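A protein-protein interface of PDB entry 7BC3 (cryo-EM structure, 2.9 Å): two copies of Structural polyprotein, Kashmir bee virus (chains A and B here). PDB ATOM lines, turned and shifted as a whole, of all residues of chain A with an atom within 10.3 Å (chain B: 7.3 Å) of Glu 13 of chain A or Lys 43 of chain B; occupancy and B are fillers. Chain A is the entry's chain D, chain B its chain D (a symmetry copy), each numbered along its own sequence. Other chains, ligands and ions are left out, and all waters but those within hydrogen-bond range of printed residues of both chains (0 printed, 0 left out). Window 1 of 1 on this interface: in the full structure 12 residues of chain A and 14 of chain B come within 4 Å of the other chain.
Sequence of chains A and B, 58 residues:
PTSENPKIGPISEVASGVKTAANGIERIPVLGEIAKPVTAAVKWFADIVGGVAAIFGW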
ATOM      1  N   PRO A   1       3.361 -34.046  28.100  1.00  0.00           N
ATOM      2  CA  PRO A   1       4.647 -34.751  28.100  1.00  0.00           C
ATOM      3  C   PRO A   1       4.798 -35.638  29.326  1.00  0.00           C
ATOM      4  O   PRO A   1       4.857 -35.133  30.447  1.00  0.00           O
ATOM      5  CB  PRO A   1       5.680 -33.614  28.106  1.00  0.00           C
ATOM      6  CG  PRO A   1       4.938 -32.412  27.651  1.00  0.00           C
ATOM      7  CD  PRO A   1       3.542 -32.588  28.146  1.00  0.00           C
ATOM      8  N   THR A   2       4.869 -36.949  29.110  1.00  0.00           N
ATOM      9  CA  THR A   2       4.882 -37.916  30.203  1.00  0.00           C
ATOM     10  C   THR A   2       6.311 -38.070  30.700  1.00  0.00           C
ATOM     11  O   THR A   2       7.163 -38.660  30.024  1.00  0.00           O
ATOM     12  CB  THR A   2       4.304 -39.251  29.756  1.00  0.00           C
ATOM     13  OG1 THR A   2       5.142 -39.832  28.749  1.00  0.00           O
ATOM     14  CG2 THR A   2       2.900 -39.050  29.206  1.00  0.00           C
ATOM     15  N   SER A   3       6.565 -37.538  31.892  1.00  0.00           N
ATOM     16  CA  SER A   3       7.877 -37.570  32.511  1.00  0.00           C
ATOM     17  C   SER A   3       7.684 -37.882  33.983  1.00  0.00           C
ATOM     18  O   SER A   3       6.857 -37.253  34.651  1.00  0.00           O
ATOM     19  CB  SER A   3       8.607 -36.235  32.349  1.00  0.00           C
ATOM     20  OG  SER A   3       9.880 -36.264  32.955  1.00  0.00           O
ATOM     21  N   GLU A   4       8.447 -38.850  34.485  1.00  0.00           N
ATOM     22  CA  GLU A   4       8.381 -39.167  35.905  1.00  0.00           C
ATOM     23  C   GLU A   4       9.240 -38.237  36.744  1.00  0.00           C
ATOM     24  O   GLU A   4       9.186 -38.309  37.977  1.00  0.00           O
ATOM     25  CB  GLU A   4       8.796 -40.617  36.143  1.00  0.00           C
ATOM     26  CG  GLU A   4       7.762 -41.612  35.680  1.00  0.00           C
ATOM     27  CD  GLU A   4       8.342 -42.985  35.455  1.00  0.00           C
ATOM     28  OE1 GLU A   4       8.513 -43.358  34.281  1.00  0.00           O
ATOM     29  OE2 GLU A   4       8.624 -43.687  36.449  1.00  0.00           O
ATOM     30  N   ASN A   5      10.027 -37.383  36.113  1.00  0.00           N
ATOM     31  CA  ASN A   5      10.725 -36.325  36.822  1.00  0.00           C
ATOM     32  C   ASN A   5       9.835 -35.097  36.895  1.00  0.00           C
ATOM     33  O   ASN A   5       9.335 -34.646  35.854  1.00  0.00           O
ATOM     34  CB  ASN A   5      12.030 -35.973  36.118  1.00  0.00           C
ATOM     35  CG  ASN A   5      12.941 -35.123  36.975  1.00  0.00           C
ATOM     36  OD1 ASN A   5      12.496 -34.187  37.638  1.00  0.00           O
ATOM     37  ND2 ASN A   5      14.227 -35.446  36.968  1.00  0.00           N
ATOM     38  N   PRO A   6       9.596 -34.530  38.080  1.00  0.00           N
ATOM     39  CA  PRO A   6       8.798 -33.297  38.138  1.00  0.00           C
ATOM     40  C   PRO A   6       9.367 -32.192  37.275  1.00  0.00           C
ATOM     41  O   PRO A   6       8.604 -31.397  36.712  1.00  0.00           O
ATOM     42  CB  PRO A   6       8.827 -32.933  39.627  1.00  0.00           C
ATOM     43  CG  PRO A   6       9.123 -34.208  40.327  1.00  0.00           C
ATOM     44  CD  PRO A   6      10.009 -34.983  39.418  1.00  0.00           C
ATOM     45  N   LYS A   7      10.689 -32.115  37.158  1.00  0.00           N
ATOM     46  CA  LYS A   7      11.348 -31.188  36.243  1.00  0.00           C
ATOM     47  C   LYS A   7      11.496 -31.902  34.908  1.00  0.00           C
ATOM     48  O   LYS A   7      12.449 -32.655  34.693  1.00  0.00           O
ATOM     49  CB  LYS A   7      12.694 -30.747  36.804  1.00  0.00           C
ATOM     50  CG  LYS A   7      13.090 -29.341  36.422  1.00  0.00           C
ATOM     51  CD  LYS A   7      14.501 -29.031  36.869  1.00  0.00           C
ATOM     52  CE  LYS A   7      14.995 -27.729  36.270  1.00  0.00           C
ATOM     53  NZ  LYS A   7      16.440 -27.502  36.545  1.00  0.00           N
ATOM     54  N   ILE A   8      10.542 -31.670  34.005  1.00  0.00           N
ATOM     55  CA  ILE A   8      10.501 -32.428  32.759  1.00  0.00           C
ATOM     56  C   ILE A   8      11.752 -32.170  31.932  1.00  0.00           C
ATOM     57  O   ILE A   8      12.213 -33.044  31.187  1.00  0.00           O
ATOM     58  CB  ILE A   8       9.221 -32.091  31.974  1.00  0.00           C
ATOM     59  CG1 ILE A   8       7.986 -32.443  32.808  1.00  0.00           C
ATOM     60  CG2 ILE A   8       9.216 -32.827  30.644  1.00  0.00           C
ATOM     61  CD1 ILE A   8       6.670 -32.057  32.175  1.00  0.00           C
ATOM     62  N   GLY A   9      12.323 -30.974  32.046  1.00  0.00           N
ATOM     63  CA  GLY A   9      13.505 -30.626  31.298  1.00  0.00           C
ATOM     64  C   GLY A   9      14.436 -29.723  32.080  1.00  0.00           C
ATOM     65  O   GLY A   9      14.062 -29.148  33.106  1.00  0.00           O
ATOM     66  N   PRO A  10      15.677 -29.580  31.608  1.00  0.00           N
ATOM     67  CA  PRO A  10      16.618 -28.701  32.315  1.00  0.00           C
ATOM     68  C   PRO A  10      16.234 -27.238  32.258  1.00  0.00           C
ATOM     69  O   PRO A  10      16.542 -26.493  33.196  1.00  0.00           O
ATOM     70  CB  PRO A  10      17.947 -28.946  31.587  1.00  0.00           C
ATOM     71  CG  PRO A  10      17.780 -30.221  30.872  1.00  0.00           C
ATOM     72  CD  PRO A  10      16.335 -30.304  30.508  1.00  0.00           C
ATOM     73  N   ILE A  11      15.571 -26.800  31.189  1.00  0.00           N
ATOM     74  CA  ILE A  11      15.358 -25.388  30.922  1.00  0.00           C
ATOM     75  C   ILE A  11      13.886 -25.149  30.617  1.00  0.00           C
ATOM     76  O   ILE A  11      13.097 -26.081  30.455  1.00  0.00           O
ATOM     77  CB  ILE A  11      16.235 -24.882  29.758  1.00  0.00           C
ATOM     78  CG1 ILE A  11      15.971 -25.691  28.489  1.00  0.00           C
ATOM     79  CG2 ILE A  11      17.701 -24.978  30.119  1.00  0.00           C
ATOM     80  CD1 ILE A  11      16.263 -24.928  27.231  1.00  0.00           C
ATOM     81  N   SER A  12      13.528 -23.872  30.536  1.00  0.00           N
ATOM     82  CA  SER A  12      12.185 -23.456  30.159  1.00  0.00           C
ATOM     83  C   SER A  12      12.135 -23.278  28.647  1.00  0.00           C
ATOM     84  O   SER A  12      12.889 -22.476  28.085  1.00  0.00           O
ATOM     85  CB  SER A  12      11.800 -22.161  30.869  1.00  0.00           C
ATOM     86  OG  SER A  12      12.497 -21.056  30.326  1.00  0.00           O
ATOM     87  N   GLU A  13      11.250 -24.023  27.993  1.00  0.00           N
ATOM     88  CA  GLU A  13      11.188 -24.003  26.541  1.00  0.00           C
ATOM     89  C   GLU A  13      10.531 -22.720  26.050  1.00  0.00           C
ATOM     90  O   GLU A  13       9.539 -22.254  26.615  1.00  0.00           O
ATOM     91  CB  GLU A  13      10.417 -25.217  26.030  1.00  0.00           C
ATOM     92  CG  GLU A  13      11.087 -26.562  26.316  1.00  0.00           C
ATOM     93  CD  GLU A  13      12.490 -26.685  25.734  1.00  0.00           C
ATOM     94  OE1 GLU A  13      12.695 -26.214  24.600  1.00  0.00           O
ATOM     95  OE2 GLU A  13      13.375 -27.280  26.383  1.00  0.00           O
ATOM     96  N   VAL A  14      11.094 -22.151  24.987  1.00  0.00           N
ATOM     97  CA  VAL A  14      10.587 -20.930  24.375  1.00  0.00           C
ATOM     98  C   VAL A  14      10.047 -21.276  22.995  1.00  0.00           C
ATOM     99  O   VAL A  14      10.697 -21.999  22.231  1.00  0.00           O
ATOM    100  CB  VAL A  14      11.678 -19.848  24.278  1.00  0.00           C
ATOM    101  CG1 VAL A  14      11.119 -18.591  23.639  1.00  0.00           C
ATOM    102  CG2 VAL A  14      12.257 -19.544  25.649  1.00  0.00           C
ATOM    103  N   ALA A  15       8.863 -20.760  22.680  1.00  0.00           N
ATOM    104  CA  ALA A  15       8.245 -21.028  21.390  1.00  0.00           C
ATOM    105  C   ALA A  15       8.905 -20.199  20.293  1.00  0.00           C
ATOM    106  O   ALA A  15       9.479 -19.138  20.544  1.00  0.00           O
ATOM    107  CB  ALA A  15       6.748 -20.731  21.445  1.00  0.00           C
ATOM    108  N   SER A  16       8.814 -20.697  19.058  1.00  0.00           N
ATOM    109  CA  SER A  16       9.504 -20.096  17.921  1.00  0.00           C
ATOM    110  C   SER A  16       8.583 -19.237  17.061  1.00  0.00           C
ATOM    111  O   SER A  16       8.818 -18.037  16.900  1.00  0.00           O
ATOM    112  CB  SER A  16      10.129 -21.194  17.055  1.00  0.00           C
ATOM    113  OG  SER A  16       9.141 -22.109  16.614  1.00  0.00           O
ATOM    114  N   GLU A  33      12.845 -18.024  14.602  1.00  0.00           N
ATOM    115  CA  GLU A  33      13.312 -19.053  15.523  1.00  0.00           C
ATOM    116  C   GLU A  33      13.332 -18.549  16.959  1.00  0.00           C
ATOM    117  O   GLU A  33      13.234 -19.352  17.894  1.00  0.00           O
ATOM    118  CB  GLU A  33      14.699 -19.533  15.101  1.00  0.00           C
ATOM    119  CG  GLU A  33      14.744 -20.129  13.710  1.00  0.00           C
ATOM    120  CD  GLU A  33      16.092 -20.731  13.378  1.00  0.00           C
ATOM    121  OE1 GLU A  33      17.029 -20.573  14.184  1.00  0.00           O
ATOM    122  OE2 GLU A  33      16.210 -21.363  12.309  1.00  0.00           O
ATOM    123  N   ILE A  34      13.449 -17.237  17.158  1.00  0.00           N
ATOM    124  CA  ILE A  34      13.384 -16.637  18.486  1.00  0.00           C
ATOM    125  C   ILE A  34      13.028 -15.165  18.335  1.00  0.00           C
ATOM    126  O   ILE A  34      13.297 -14.541  17.304  1.00  0.00           O
ATOM    127  CB  ILE A  34      14.702 -16.799  19.278  1.00  0.00           C
ATOM    128  CG1 ILE A  34      14.492 -16.402  20.744  1.00  0.00           C
ATOM    129  CG2 ILE A  34      15.794 -15.941  18.644  1.00  0.00           C
ATOM    130  CD1 ILE A  34      13.562 -17.296  21.527  1.00  0.00           C
ATOM    131  N   THR B  39       3.962 -38.592  19.294  1.00  0.00           N
ATOM    132  CA  THR B  39       3.082 -37.471  19.588  1.00  0.00           C
ATOM    133  C   THR B  39       3.875 -36.443  20.385  1.00  0.00           C
ATOM    134  O   THR B  39       5.073 -36.610  20.629  1.00  0.00           O
ATOM    135  CB  THR B  39       1.844 -37.931  20.369  1.00  0.00           C
ATOM    136  OG1 THR B  39       2.252 -38.751  21.469  1.00  0.00           O
ATOM    137  CG2 THR B  39       0.894 -38.713  19.487  1.00  0.00           C
ATOM    138  N   ALA B  40       3.193 -35.381  20.810  1.00  0.00           N
ATOM    139  CA  ALA B  40       3.784 -34.429  21.739  1.00  0.00           C
ATOM    140  C   ALA B  40       3.930 -34.994  23.145  1.00  0.00           C
ATOM    141  O   ALA B  40       4.391 -34.273  24.036  1.00  0.00           O
ATOM    142  CB  ALA B  40       2.946 -33.153  21.777  1.00  0.00           C
ATOM    143  N   ALA B  41       3.550 -36.256  23.365  1.00  0.00           N
ATOM    144  CA  ALA B  41       3.772 -36.891  24.657  1.00  0.00           C
ATOM    145  C   ALA B  41       5.249 -37.086  24.950  1.00  0.00           C
ATOM    146  O   ALA B  41       5.632 -37.171  26.122  1.00  0.00           O
ATOM    147  CB  ALA B  41       3.060 -38.242  24.706  1.00  0.00           C
ATOM    148  N   VAL B  42       6.078 -37.169  23.924  1.00  0.00           N
ATOM    149  CA  VAL B  42       7.519 -37.300  24.084  1.00  0.00           C
ATOM    150  C   VAL B  42       8.131 -35.908  24.065  1.00  0.00           C
ATOM    151  O   VAL B  42       7.717 -35.040  23.289  1.00  0.00           O
ATOM    152  CB  VAL B  42       8.110 -38.197  22.983  1.00  0.00           C
ATOM    153  CG1 VAL B  42       9.562 -38.500  23.266  1.00  0.00           C
ATOM    154  CG2 VAL B  42       7.314 -39.485  22.885  1.00  0.00           C
ATOM    155  N   LYS B  43       9.124 -35.696  24.926  1.00  0.00           N
ATOM    156  CA  LYS B  43       9.630 -34.347  25.150  1.00  0.00           C
ATOM    157  C   LYS B  43      10.307 -33.791  23.904  1.00  0.00           C
ATOM    158  O   LYS B  43       9.976 -32.693  23.446  1.00  0.00           O
ATOM    159  CB  LYS B  43      10.594 -34.348  26.335  1.00  0.00           C
ATOM    160  CG  LYS B  43      11.223 -33.002  26.631  1.00  0.00           C
ATOM    161  CD  LYS B  43      10.192 -31.987  27.058  1.00  0.00           C
ATOM    162  CE  LYS B  43      10.848 -30.690  27.479  1.00  0.00           C
ATOM    163  NZ  LYS B  43      11.143 -29.818  26.316  1.00  0.00           N
ATOM    164  N   TRP B  44      11.266 -34.529  23.345  1.00  0.00           N
ATOM    165  CA  TRP B  44      12.002 -34.010  22.196  1.00  0.00           C
ATOM    166  C   TRP B  44      11.107 -33.906  20.966  1.00  0.00           C
ATOM    167  O   TRP B  44      11.249 -32.972  20.168  1.00  0.00           O
ATOM    168  CB  TRP B  44      13.224 -34.884  21.910  1.00  0.00           C
ATOM    169  CG  TRP B  44      12.934 -36.339  21.757  1.00  0.00           C
ATOM    170  CD1 TRP B  44      12.895 -37.272  22.746  1.00  0.00           C
ATOM    171  CD2 TRP B  44      12.665 -37.035  20.538  1.00  0.00           C
ATOM    172  NE1 TRP B  44      12.608 -38.507  22.221  1.00  0.00           N
ATOM    173  CE2 TRP B  44      12.463 -38.387  20.865  1.00  0.00           C
ATOM    174  CE3 TRP B  44      12.571 -36.645  19.199  1.00  0.00           C
ATOM    175  CZ2 TRP B  44      12.173 -39.350  19.906  1.00  0.00           C
ATOM    176  CZ3 TRP B  44      12.282 -37.602  18.251  1.00  0.00           C
ATOM    177  CH2 TRP B  44      12.087 -38.937  18.608  1.00  0.00           C
ATOM    178  N   PHE B  45      10.168 -34.835  20.802  1.00  0.00           N
ATOM    179  CA  PHE B  45       9.268 -34.760  19.657  1.00  0.00           C
ATOM    180  C   PHE B  45       8.335 -33.564  19.773  1.00  0.00           C
ATOM    181  O   PHE B  45       8.042 -32.894  18.772  1.00  0.00           O
ATOM    182  CB  PHE B  45       8.468 -36.052  19.534  1.00  0.00           C
ATOM    183  CG  PHE B  45       7.748 -36.189  18.229  1.00  0.00           C
ATOM    184  CD1 PHE B  45       8.409 -36.644  17.105  1.00  0.00           C
ATOM    185  CD2 PHE B  45       6.412 -35.851  18.123  1.00  0.00           C
ATOM    186  CE1 PHE B  45       7.751 -36.766  15.904  1.00  0.00           C
ATOM    187  CE2 PHE B  45       5.750 -35.971  16.925  1.00  0.00           C
ATOM    188  CZ  PHE B  45       6.419 -36.429  15.814  1.00  0.00           C
ATOM    189  N   ALA B  46       7.843 -33.291  20.981  1.00  0.00           N
ATOM    190  CA  ALA B  46       7.064 -32.080  21.206  1.00  0.00           C
ATOM    191  C   ALA B  46       7.904 -30.841  20.941  1.00  0.00           C
ATOM    192  O   ALA B  46       7.425 -29.871  20.346  1.00  0.00           O
ATOM    193  CB  ALA B  46       6.523 -32.067  22.633  1.00  0.00           C
ATOM    194  N   ASP B  47       9.163 -30.860  21.375  1.00  0.00           N
ATOM    195  CA  ASP B  47      10.069 -29.754  21.094  1.00  0.00           C
ATOM    196  C   ASP B  47      10.175 -29.503  19.598  1.00  0.00           C
ATOM    197  O   ASP B  47      10.157 -28.353  19.147  1.00  0.00           O
ATOM    198  CB  ASP B  47      11.444 -30.061  21.678  1.00  0.00           C
ATOM    199  CG  ASP B  47      11.521 -29.800  23.167  1.00  0.00           C
ATOM    200  OD1 ASP B  47      10.515 -30.022  23.867  1.00  0.00           O
ATOM    201  OD2 ASP B  47      12.604 -29.393  23.636  1.00  0.00           O
ATOM    202  N   ILE B  48      10.286 -30.572  18.812  1.00  0.00           N
ATOM    203  CA  ILE B  48      10.439 -30.422  17.367  1.00  0.00           C
ATOM    204  C   ILE B  48       9.155 -29.883  16.751  1.00  0.00           C
ATOM    205  O   ILE B  48       9.142 -28.810  16.138  1.00  0.00           O
ATOM    206  CB  ILE B  48      10.837 -31.758  16.720  1.00  0.00           C
ATOM    207  CG1 ILE B  48      12.134 -32.296  17.329  1.00  0.00           C
ATOM    208  CG2 ILE B  48      10.988 -31.583  15.219  1.00  0.00           C
ATOM    209  CD1 ILE B  48      13.381 -31.692  16.760  1.00  0.00           C
ATOM    210  N   VAL B  49       8.057 -30.626  16.901  1.00  0.00           N
ATOM    211  CA  VAL B  49       6.822 -30.276  16.206  1.00  0.00           C
ATOM    212  C   VAL B  49       6.186 -29.000  16.727  1.00  0.00           C
ATOM    213  O   VAL B  49       5.365 -28.400  16.025  1.00  0.00           O
ATOM    214  CB  VAL B  49       5.807 -31.432  16.291  1.00  0.00           C
ATOM    215  CG1 VAL B  49       6.421 -32.706  15.744  1.00  0.00           C
ATOM    216  CG2 VAL B  49       5.336 -31.623  17.718  1.00  0.00           C
ATOM    217  N   VAL B  52      10.246 -25.210  19.153  1.00  0.00           N
ATOM    218  CA  VAL B  52      10.828 -24.394  20.204  1.00  0.00           C
ATOM    219  C   VAL B  52      12.170 -23.847  19.722  1.00  0.00           C
ATOM    220  O   VAL B  52      12.769 -24.337  18.758  1.00  0.00           O
ATOM    221  CB  VAL B  52      10.989 -25.178  21.515  1.00  0.00           C
ATOM    222  CG1 VAL B  52       9.635 -25.622  22.029  1.00  0.00           C
ATOM    223  CG2 VAL B  52      11.912 -26.366  21.331  1.00  0.00           C
ATOM    224  N   ALA B  53      12.641 -22.808  20.407  1.00  0.00           N
ATOM    225  CA  ALA B  53      13.850 -22.116  19.991  1.00  0.00           C
ATOM    226  C   ALA B  53      15.125 -22.845  20.387  1.00  0.00           C
ATOM    227  O   ALA B  53      16.212 -22.414  19.989  1.00  0.00           O
ATOM    228  CB  ALA B  53      13.867 -20.707  20.583  1.00  0.00           C
ATOM    229  N   ALA B  54      15.025 -23.935  21.147  1.00  0.00           N
ATOM    230  CA  ALA B  54      16.220 -24.633  21.599  1.00  0.00           C
ATOM    231  C   ALA B  54      16.744 -25.607  20.554  1.00  0.00           C
ATOM    232  O   ALA B  54      17.959 -25.801  20.449  1.00  0.00           O
ATOM    233  CB  ALA B  54      15.933 -25.372  22.903  1.00  0.00           C
ATOM    234  N   ILE B  55      15.853 -26.225  19.775  1.00  0.00           N
ATOM    235  CA  ILE B  55      16.282 -27.120  18.710  1.00  0.00           C
ATOM    236  C   ILE B  55      17.065 -26.396  17.629  1.00  0.00           C
ATOM    237  O   ILE B  55      17.697 -27.047  16.790  1.00  0.00           O
ATOM    238  CB  ILE B  55      15.067 -27.835  18.084  1.00  0.00           C
ATOM    239  CG1 ILE B  55      14.045 -26.822  17.575  1.00  0.00           C
ATOM    240  CG2 ILE B  55      14.413 -28.749  19.098  1.00  0.00           C
ATOM    241  CD1 ILE B  55      13.206 -27.337  16.439  1.00  0.00           C
ATOM    242  N   TRP B  58      19.050 -21.651  20.220  1.00  0.00           N
ATOM    243  CA  TRP B  58      18.792 -20.393  20.903  1.00  0.00           C
ATOM    244  C   TRP B  58      18.261 -20.644  22.304  1.00  0.00           C
ATOM    245  O   TRP B  58      17.361 -21.461  22.497  1.00  0.00           O
ATOM    246  CB  TRP B  58      17.796 -19.550  20.112  1.00  0.00           C
ATOM    247  CG  TRP B  58      18.190 -19.342  18.695  1.00  0.00           C
ATOM    248  CD1 TRP B  58      17.449 -19.634  17.591  1.00  0.00           C
ATOM    249  CD2 TRP B  58      19.422 -18.793  18.219  1.00  0.00           C
ATOM    250  NE1 TRP B  58      18.143 -19.302  16.456  1.00  0.00           N
ATOM    251  CE2 TRP B  58      19.357 -18.783  16.815  1.00  0.00           C
ATOM    252  CE3 TRP B  58      20.572 -18.308  18.845  1.00  0.00           C
ATOM    253  CZ2 TRP B  58      20.399 -18.307  16.025  1.00  0.00           C
ATOM    254  CZ3 TRP B  58      21.603 -17.838  18.061  1.00  0.00           C
ATOM    255  CH2 TRP B  58      21.511 -17.841  16.667  1.00  0.00           C
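The indole nitrogen (NE1) of Trp 58 of chain B lies within hydrogen-bond range of the side-chain carboxylate (OE1) of Glu 33 of chain A, 2.8 Å away.
The side-chain carboxylate (OE2) of Glu 13 of chain A lies within salt-bridge range of the side-chain amino group (NZ) of Lys 43 of chain B.
N of Thr 2 of chain A is in hydrogen-bond range of O of Ala 41 of chain B (3.1 Å).
The backbone carbonyl oxygen of Val 14 of chain A lies within hydrogen-bond range of the backbone NH of Ala 53 of chain B (2.8 Å).
OE1 of Glu 13 of chain A lies close to OD2 of Asp 47 of chain B (3.3 Å).
The side-chain carboxylate (OD1) of Asp 47 of chain B lies within salt-bridge range of the side-chain amino group (NZ) of Lys 43 of chain B, 2.5 Å away.
The backbone NH (N) of Ala 41 of chain B lies close to the side-chain hydroxyl (OG1) of Thr 39 of chain B (3.4 Å).
O of Ala 53 of chain B is in hydrogen-bond range of N of Trp 58 of chain B.
O of Asp 47 of chain B is in hydrogen-bond range of N of Val 52 of chain B, at 3.1 Å.
Pro 1 of chain A touches Ala 41 of chain B (CA to O, 3.3 Å).
CD of Lys 43 of chain B touches CG2 of Ile 8 of chain A, 3.8 Å away.
Glu 13 of chain A touches Val 52 of chain B.
CB of Ala 54 of chain B touches OE1 of Glu 13 of chain A, at 3.8 Å.
Val 52 of chain B touches Val 14 of chain A.
O of Glu 33 of chain A touches CB of Ala 53 of chain B (3.1 Å).
Ala 53 of chain B touches Ile 34 of chain A.
Of the printed residues of chain B, Thr 2 of chain A touches Ala 41.
Of chain B, only Lys 43 (3.3 Å), Asp 47 (3.3 Å), Val 52 (3.4 Å) and Ala 54 (3.8 Å) come within 4 Å of Glu 13 of chain A.
Printed residues of chain B within 4 Å of Ile 34 of chain A: Ala 53 (3.6 Å).
No residue of chain A comes within 4 Å of Val 42 of chain B.
Phe 45 of chain B touches none of the printed residues of chain A.
No residue of chain A comes within 4 Å of Ala 46 of chain B.
Asp 47 of chain B touches one residue of chain A.
Val 52 of chain B touches just these residues of chain A: Glu 13 and Val 14.
Of the printed residues of chain A, Ala 53 of chain B touches Val 14 (2.8 Å), Glu 33 (3.1 Å) and Ile 34 (3.6 Å).
Of the printed residues of chain A, Ala 54 of chain B touches Glu 13 (3.8 Å).
Of the printed residues of chain A, Trp 58 of chain B touches Glu 33 (2.8 Å).
Of the 18 printed residues of chain A, 7 touch a printed residue of chain B.
Printed residues of chain A that touch a printed residue of chain B: Pro 1, Thr 2, Ile 8, Glu 13, Val 14, Glu 33 and Ile 34.
Hydrophobic or aromatic side chains of chain A that line the printed part of chain B: Ile 8 and Ile 34.
Of the 16 printed residues of chain B, 7 touch a printed residue of chain A.
Hydrophobic or aromatic side chains of chain B that line the printed part of chain A: Val 52, Ala 53, Ala 54 and Trp 58.
Among the printed residues, 12 pairs touch across the chains.
Among the printed residues, Asp or Glu carboxylates within 4 Å of a Lys or Arg side-chain nitrogen of the other chain: Glu 13 of chain A with Lys 43 of chain B.
No position is printed for both chains.
Of the 12 pairs that touch across the chains among the printed residues, none has its exchanged pair printed and touching as well.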
